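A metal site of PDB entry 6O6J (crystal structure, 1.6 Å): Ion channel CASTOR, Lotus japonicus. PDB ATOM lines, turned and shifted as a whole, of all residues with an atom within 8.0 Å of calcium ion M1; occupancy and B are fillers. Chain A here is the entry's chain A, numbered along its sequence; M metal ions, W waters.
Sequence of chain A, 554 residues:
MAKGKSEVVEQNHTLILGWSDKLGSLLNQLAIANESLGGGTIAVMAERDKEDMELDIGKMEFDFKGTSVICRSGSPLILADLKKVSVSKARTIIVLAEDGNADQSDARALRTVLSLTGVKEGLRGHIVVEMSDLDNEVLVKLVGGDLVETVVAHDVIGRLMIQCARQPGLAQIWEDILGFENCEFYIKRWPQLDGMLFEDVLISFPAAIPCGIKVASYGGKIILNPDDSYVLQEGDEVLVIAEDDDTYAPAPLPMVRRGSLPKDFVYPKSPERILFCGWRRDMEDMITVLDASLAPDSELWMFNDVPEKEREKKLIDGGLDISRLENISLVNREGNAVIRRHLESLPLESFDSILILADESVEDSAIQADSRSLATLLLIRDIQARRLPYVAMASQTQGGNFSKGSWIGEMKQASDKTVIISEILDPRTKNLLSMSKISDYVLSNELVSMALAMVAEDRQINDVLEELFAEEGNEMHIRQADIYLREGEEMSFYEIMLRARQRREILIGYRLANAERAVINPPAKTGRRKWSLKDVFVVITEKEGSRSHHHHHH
The side-chain amide oxygen (OE1) of Gln 29 is in hydrogen-bond range of the backbone NH (N) of Phe 180 (2.8 Å).
N of Glu 243 lies within hydrogen-bond range of SG of Cys 183.
The side-chain carboxylate (OE2) of Glu 184 sits close to the side-chain hydroxyl (OH) of Tyr 186 (2.5 Å).
N of Glu 184 lies within hydrogen-bond range of O of Ala 242, 2.9 Å away.
Calcium ion M1 is bound by O of Phe 180 (2.3 Å).
O of Glu 243 is bound to calcium ion M1 (2.3 Å).
O of Asn 182 binds calcium ion M1 (2.3 Å).
Water W2 binds calcium ion M1 (2.4 Å).
The side-chain carboxylate (OE2) of Glu 184 binds calcium ion M1, at 2.4 Å.
Water W1 is bound to calcium ion M1 (2.5 Å).
Calcium ion M1 is bound by the side-chain carboxylate (OE1) of Glu 184, 2.6 Å away.
Glu 181 touches calcium ion M1.
Within 4 Å of calcium ion M1: Phe 180, Glu 181, Asn 182, Glu 184 and Glu 243.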
ATOM      1  N   GLN A  29      -0.251   9.429 -10.161  1.00  0.00           N
ATOM      2  CA  GLN A  29       0.592   8.957  -9.060  1.00  0.00           C
ATOM      3  C   GLN A  29      -0.126   7.944  -8.189  1.00  0.00           C
ATOM      4  O   GLN A  29       0.466   6.931  -7.788  1.00  0.00           O
ATOM      5  CB  GLN A  29       1.028  10.126  -8.178  1.00  0.00           C
ATOM      6  CG  GLN A  29       2.008  11.018  -8.857  1.00  0.00           C
ATOM      7  CD  GLN A  29       3.315  10.274  -9.136  1.00  0.00           C
ATOM      8  OE1 GLN A  29       3.843   9.543  -8.252  1.00  0.00           O
ATOM      9  NE2 GLN A  29       3.816  10.382 -10.350  1.00  0.00           N
ATOM     10  N   ILE A  32      -0.390   4.617  -9.866  1.00  0.00           N
ATOM     11  CA  ILE A  32       0.878   3.871  -9.790  1.00  0.00           C
ATOM     12  C   ILE A  32       1.062   3.263  -8.397  1.00  0.00           C
ATOM     13  O   ILE A  32       1.462   2.102  -8.263  1.00  0.00           O
ATOM     14  CB  ILE A  32       2.049   4.786 -10.187  1.00  0.00           C
ATOM     15  CG1 ILE A  32       1.926   5.252 -11.649  1.00  0.00           C
ATOM     16  CG2 ILE A  32       3.376   4.027 -10.057  1.00  0.00           C
ATOM     17  CD1 ILE A  32       2.835   6.491 -11.954  1.00  0.00           C
ATOM     18  N   ALA A  33       0.780   4.046  -7.350  1.00  0.00           N
ATOM     19  CA  ALA A  33       0.892   3.536  -5.983  1.00  0.00           C
ATOM     20  C   ALA A  33      -0.042   2.360  -5.726  1.00  0.00           C
ATOM     21  O   ALA A  33       0.314   1.419  -5.003  1.00  0.00           O
ATOM     22  CB  ALA A  33       0.613   4.678  -4.968  1.00  0.00           C
ATOM     23  N   GLU A  35      -1.128   0.177  -7.938  1.00  0.00           N
ATOM     24  CA  GLU A  35      -1.036  -0.925  -8.907  1.00  0.00           C
ATOM     25  C   GLU A  35      -0.708  -2.251  -8.225  1.00  0.00           C
ATOM     26  O   GLU A  35      -1.254  -3.304  -8.616  1.00  0.00           O
ATOM     27  CB  GLU A  35       0.011  -0.594  -9.954  1.00  0.00           C
ATOM     28  CG  GLU A  35       0.077  -1.657 -11.069  1.00  0.00           C
ATOM     29  CD  GLU A  35       1.122  -1.328 -12.103  1.00  0.00           C
ATOM     30  OE1 GLU A  35       2.102  -0.625 -11.764  1.00  0.00           O
ATOM     31  OE2 GLU A  35       0.951  -1.749 -13.268  1.00  0.00           O
ATOM     32  N   ASP A 176      12.568  10.988  -9.743  1.00  0.00           N
ATOM     33  CA  ASP A 176      12.468   9.543  -9.562  1.00  0.00           C
ATOM     34  C   ASP A 176      11.987   9.195  -8.146  1.00  0.00           C
ATOM     35  O   ASP A 176      11.113   8.342  -7.964  1.00  0.00           O
ATOM     36  CB  ASP A 176      13.833   8.908  -9.832  1.00  0.00           C
ATOM     37  CG  ASP A 176      14.109   8.733 -11.312  1.00  0.00           C
ATOM     38  OD1 ASP A 176      13.245   9.100 -12.132  1.00  0.00           O
ATOM     39  OD2 ASP A 176      15.202   8.233 -11.652  1.00  0.00           O
ATOM     40  N   ILE A 177      12.554   9.846  -7.135  1.00  0.00           N
ATOM     41  CA  ILE A 177      12.279   9.449  -5.741  1.00  0.00           C
ATOM     42  C   ILE A 177      10.951  10.006  -5.225  1.00  0.00           C
ATOM     43  O   ILE A 177      10.271   9.357  -4.414  1.00  0.00           O
ATOM     44  CB  ILE A 177      13.455   9.892  -4.860  1.00  0.00           C
ATOM     45  CG1 ILE A 177      14.665   9.026  -5.180  1.00  0.00           C
ATOM     46  CG2 ILE A 177      13.128   9.744  -3.375  1.00  0.00           C
ATOM     47  CD1 ILE A 177      15.886   9.479  -4.370  1.00  0.00           C
ATOM     48  N   GLY A 179       8.172  10.632  -6.940  1.00  0.00           N
ATOM     49  CA  GLY A 179       7.033  10.023  -7.599  1.00  0.00           C
ATOM     50  C   GLY A 179       7.080   8.506  -7.426  1.00  0.00           C
ATOM     51  O   GLY A 179       8.068   7.953  -6.943  1.00  0.00           O
ATOM     52  N   PHE A 180       5.976   7.852  -7.799  1.00  0.00           N
ATOM     53  CA  PHE A 180       5.881   6.417  -7.573  1.00  0.00           C
ATOM     54  C   PHE A 180       6.471   5.576  -8.686  1.00  0.00           C
ATOM     55  O   PHE A 180       6.662   4.371  -8.477  1.00  0.00           O
ATOM     56  CB  PHE A 180       4.433   5.997  -7.301  1.00  0.00           C
ATOM     57  CG  PHE A 180       4.016   6.252  -5.862  1.00  0.00           C
ATOM     58  CD1 PHE A 180       4.401   5.366  -4.858  1.00  0.00           C
ATOM     59  CD2 PHE A 180       3.331   7.420  -5.495  1.00  0.00           C
ATOM     60  CE1 PHE A 180       4.079   5.602  -3.496  1.00  0.00           C
ATOM     61  CE2 PHE A 180       3.016   7.652  -4.139  1.00  0.00           C
ATOM     62  CZ  PHE A 180       3.390   6.764  -3.145  1.00  0.00           C
ATOM     63  N   GLU A 181       6.786   6.152  -9.835  1.00  0.00           N
ATOM     64  CA  GLU A 181       7.622   5.401 -10.778  1.00  0.00           C
ATOM     65  C   GLU A 181       8.986   5.175 -10.167  1.00  0.00           C
ATOM     66  O   GLU A 181       9.423   5.941  -9.301  1.00  0.00           O
ATOM     67  CB  GLU A 181       7.763   6.144 -12.119  1.00  0.00           C
ATOM     68  CG  GLU A 181       6.517   6.104 -12.961  1.00  0.00           C
ATOM     69  CD  GLU A 181       6.661   6.898 -14.251  1.00  0.00           C
ATOM     70  OE1 GLU A 181       7.644   7.655 -14.385  1.00  0.00           O
ATOM     71  OE2 GLU A 181       5.778   6.769 -15.130  1.00  0.00           O
ATOM     72  N   ASN A 182       9.636   4.090 -10.576  1.00  0.00           N
ATOM     73  CA  ASN A 182      10.990   3.743 -10.075  1.00  0.00           C
ATOM     74  C   ASN A 182      10.882   3.492  -8.564  1.00  0.00           C
ATOM     75  O   ASN A 182       9.934   2.830  -8.121  1.00  0.00           O
ATOM     76  CB  ASN A 182      11.965   4.839 -10.506  1.00  0.00           C
ATOM     77  CG  ASN A 182      12.165   4.821 -12.021  1.00  0.00           C
ATOM     78  OD1 ASN A 182      12.022   5.834 -12.692  1.00  0.00           O
ATOM     79  ND2 ASN A 182      12.419   3.642 -12.552  1.00  0.00           N
ATOM     80  N   CYS A 183      11.847   3.967  -7.767  1.00  0.00           N
ATOM     81  CA  CYS A 183      11.915   3.668  -6.341  1.00  0.00           C
ATOM     82  C   CYS A 183      11.573   4.890  -5.504  1.00  0.00           C
ATOM     83  O   CYS A 183      11.656   6.040  -5.975  1.00  0.00           O
ATOM     84  CB  CYS A 183      13.303   3.157  -5.938  1.00  0.00           C
ATOM     85  SG  CYS A 183      13.657   1.542  -6.627  1.00  0.00           S
ATOM     86  N   GLU A 184      11.179   4.651  -4.254  1.00  0.00           N
ATOM     87  CA  GLU A 184      10.740   5.740  -3.373  1.00  0.00           C
ATOM     88  C   GLU A 184      10.804   5.259  -1.917  1.00  0.00           C
ATOM     89  O   GLU A 184      11.125   4.100  -1.647  1.00  0.00           O
ATOM     90  CB  GLU A 184       9.333   6.229  -3.782  1.00  0.00           C
ATOM     91  CG  GLU A 184       8.232   5.100  -3.794  1.00  0.00           C
ATOM     92  CD  GLU A 184       8.122   4.328  -5.102  1.00  0.00           C
ATOM     93  OE1 GLU A 184       8.717   4.709  -6.135  1.00  0.00           O
ATOM     94  OE2 GLU A 184       7.418   3.283  -5.095  1.00  0.00           O
ATOM     95  N   PHE A 185      10.506   6.170  -0.983  1.00  0.00           N
ATOM     96  CA  PHE A 185      10.601   5.860   0.447  1.00  0.00           C
ATOM     97  C   PHE A 185       9.394   5.056   0.944  1.00  0.00           C
ATOM     98  O   PHE A 185       8.233   5.376   0.660  1.00  0.00           O
ATOM     99  CB  PHE A 185      10.690   7.145   1.271  1.00  0.00           C
ATOM    100  CG  PHE A 185      12.019   7.866   1.161  1.00  0.00           C
ATOM    101  CD1 PHE A 185      13.170   7.311   1.720  1.00  0.00           C
ATOM    102  CD2 PHE A 185      12.101   9.103   0.539  1.00  0.00           C
ATOM    103  CE1 PHE A 185      14.406   7.984   1.636  1.00  0.00           C
ATOM    104  CE2 PHE A 185      13.333   9.758   0.431  1.00  0.00           C
ATOM    105  CZ  PHE A 185      14.480   9.209   0.983  1.00  0.00           C
ATOM    106  N   TYR A 186       9.696   4.020   1.732  1.00  0.00           N
ATOM    107  CA  TYR A 186       8.699   3.218   2.432  1.00  0.00           C
ATOM    108  C   TYR A 186       9.128   2.993   3.875  1.00  0.00           C
ATOM    109  O   TYR A 186      10.313   2.838   4.174  1.00  0.00           O
ATOM    110  CB  TYR A 186       8.481   1.831   1.788  1.00  0.00           C
ATOM    111  CG  TYR A 186       7.812   1.949   0.443  1.00  0.00           C
ATOM    112  CD1 TYR A 186       6.445   2.149   0.351  1.00  0.00           C
ATOM    113  CD2 TYR A 186       8.548   1.909  -0.731  1.00  0.00           C
ATOM    114  CE1 TYR A 186       5.808   2.304  -0.888  1.00  0.00           C
ATOM    115  CE2 TYR A 186       7.925   2.046  -1.992  1.00  0.00           C
ATOM    116  CZ  TYR A 186       6.545   2.257  -2.042  1.00  0.00           C
ATOM    117  OH  TYR A 186       5.914   2.465  -3.245  1.00  0.00           O
ATOM    118  N   ALA A 242      12.800   1.701  -1.913  1.00  0.00           N
ATOM    119  CA  ALA A 242      12.507   0.448  -2.607  1.00  0.00           C
ATOM    120  C   ALA A 242      11.581   0.702  -3.787  1.00  0.00           C
ATOM    121  O   ALA A 242      10.983   1.792  -3.925  1.00  0.00           O
ATOM    122  CB  ALA A 242      11.866  -0.599  -1.666  1.00  0.00           C
ATOM    123  N   GLU A 243      11.443  -0.324  -4.649  1.00  0.00           N
ATOM    124  CA  GLU A 243      10.649  -0.160  -5.869  1.00  0.00           C
ATOM    125  C   GLU A 243       9.150  -0.034  -5.597  1.00  0.00           C
ATOM    126  O   GLU A 243       8.443   0.709  -6.313  1.00  0.00           O
ATOM    127  CB  GLU A 243      10.916  -1.340  -6.811  1.00  0.00           C
ATOM    128  CG  GLU A 243      10.285  -1.098  -8.177  1.00  0.00           C
ATOM    129  CD  GLU A 243      10.713  -2.143  -9.223  1.00  0.00           C
ATOM    130  OE1 GLU A 243      10.690  -3.352  -8.921  1.00  0.00           O
ATOM    131  OE2 GLU A 243      11.070  -1.730 -10.353  1.00  0.00           O
ATOM    132  N   ASP A 244       8.639  -0.738  -4.590  1.00  0.00           N
ATOM    133  CA  ASP A 244       7.223  -0.702  -4.254  1.00  0.00           C
ATOM    134  C   ASP A 244       7.119  -1.169  -2.809  1.00  0.00           C
ATOM    135  O   ASP A 244       8.103  -1.628  -2.215  1.00  0.00           O
ATOM    136  CB  ASP A 244       6.399  -1.571  -5.240  1.00  0.00           C
ATOM    137  CG  ASP A 244       4.996  -1.000  -5.523  1.00  0.00           C
ATOM    138  OD1 ASP A 244       4.395  -0.379  -4.647  1.00  0.00           O
ATOM    139  OD2 ASP A 244       4.481  -1.184  -6.659  1.00  0.00           O
ATOM    140  N   ASP A 245       5.914  -1.095  -2.258  1.00  0.00           N
ATOM    141  CA  ASP A 245       5.782  -1.395  -0.837  1.00  0.00           C
ATOM    142  C   ASP A 245       6.011  -2.864  -0.533  1.00  0.00           C
ATOM    143  O   ASP A 245       6.280  -3.204   0.624  1.00  0.00           O
ATOM    144  CB  ASP A 245       4.388  -0.996  -0.324  1.00  0.00           C
ATOM    145  CG  ASP A 245       3.258  -1.654  -1.117  1.00  0.00           C
ATOM    146  OD1 ASP A 245       2.900  -1.137  -2.193  1.00  0.00           O
ATOM    147  OD2 ASP A 245       2.725  -2.714  -0.685  1.00  0.00           O
ATOM    148  N   THR A 247       8.064  -5.152  -2.539  1.00  0.00           N
ATOM    149  CA  THR A 247       9.073  -5.772  -3.381  1.00  0.00           C
ATOM    150  C   THR A 247      10.321  -6.185  -2.618  1.00  0.00           C
ATOM    151  O   THR A 247      11.266  -6.692  -3.236  1.00  0.00           O
ATOM    152  CB  THR A 247       9.482  -4.816  -4.526  1.00  0.00           C
ATOM    153  OG1 THR A 247       9.932  -3.583  -3.954  1.00  0.00           O
ATOM    154  CG2 THR A 247       8.320  -4.558  -5.528  1.00  0.00           C
ATOM    155  N   MET A 454       2.724  11.141  -2.151  1.00  0.00           N
ATOM    156  CA  MET A 454       3.577  10.476  -1.157  1.00  0.00           C
ATOM    157  C   MET A 454       3.009  10.644   0.241  1.00  0.00           C
ATOM    158  O   MET A 454       2.893   9.675   1.024  1.00  0.00           O
ATOM    159  CB  MET A 454       4.992  11.046  -1.194  1.00  0.00           C
ATOM    160  CG  MET A 454       5.781  10.639  -2.384  1.00  0.00           C
ATOM    161  SD  MET A 454       6.316   8.904  -2.178  1.00  0.00           S
ATOM    162  CE  MET A 454       6.559   8.453  -3.915  1.00  0.00           C
HETATM  163 CA    CA M   1       7.738   2.641  -7.389  1.00  0.00          CA
HETATM  164 CA    CA M   2       2.037   0.024  -4.107  1.00  0.00          CA
HETATM  165  O   HOH W   1       5.375   1.863  -7.019  1.00  0.00           O
HETATM  166  O   HOH W   2       7.457   1.297  -9.341  1.00  0.00           O
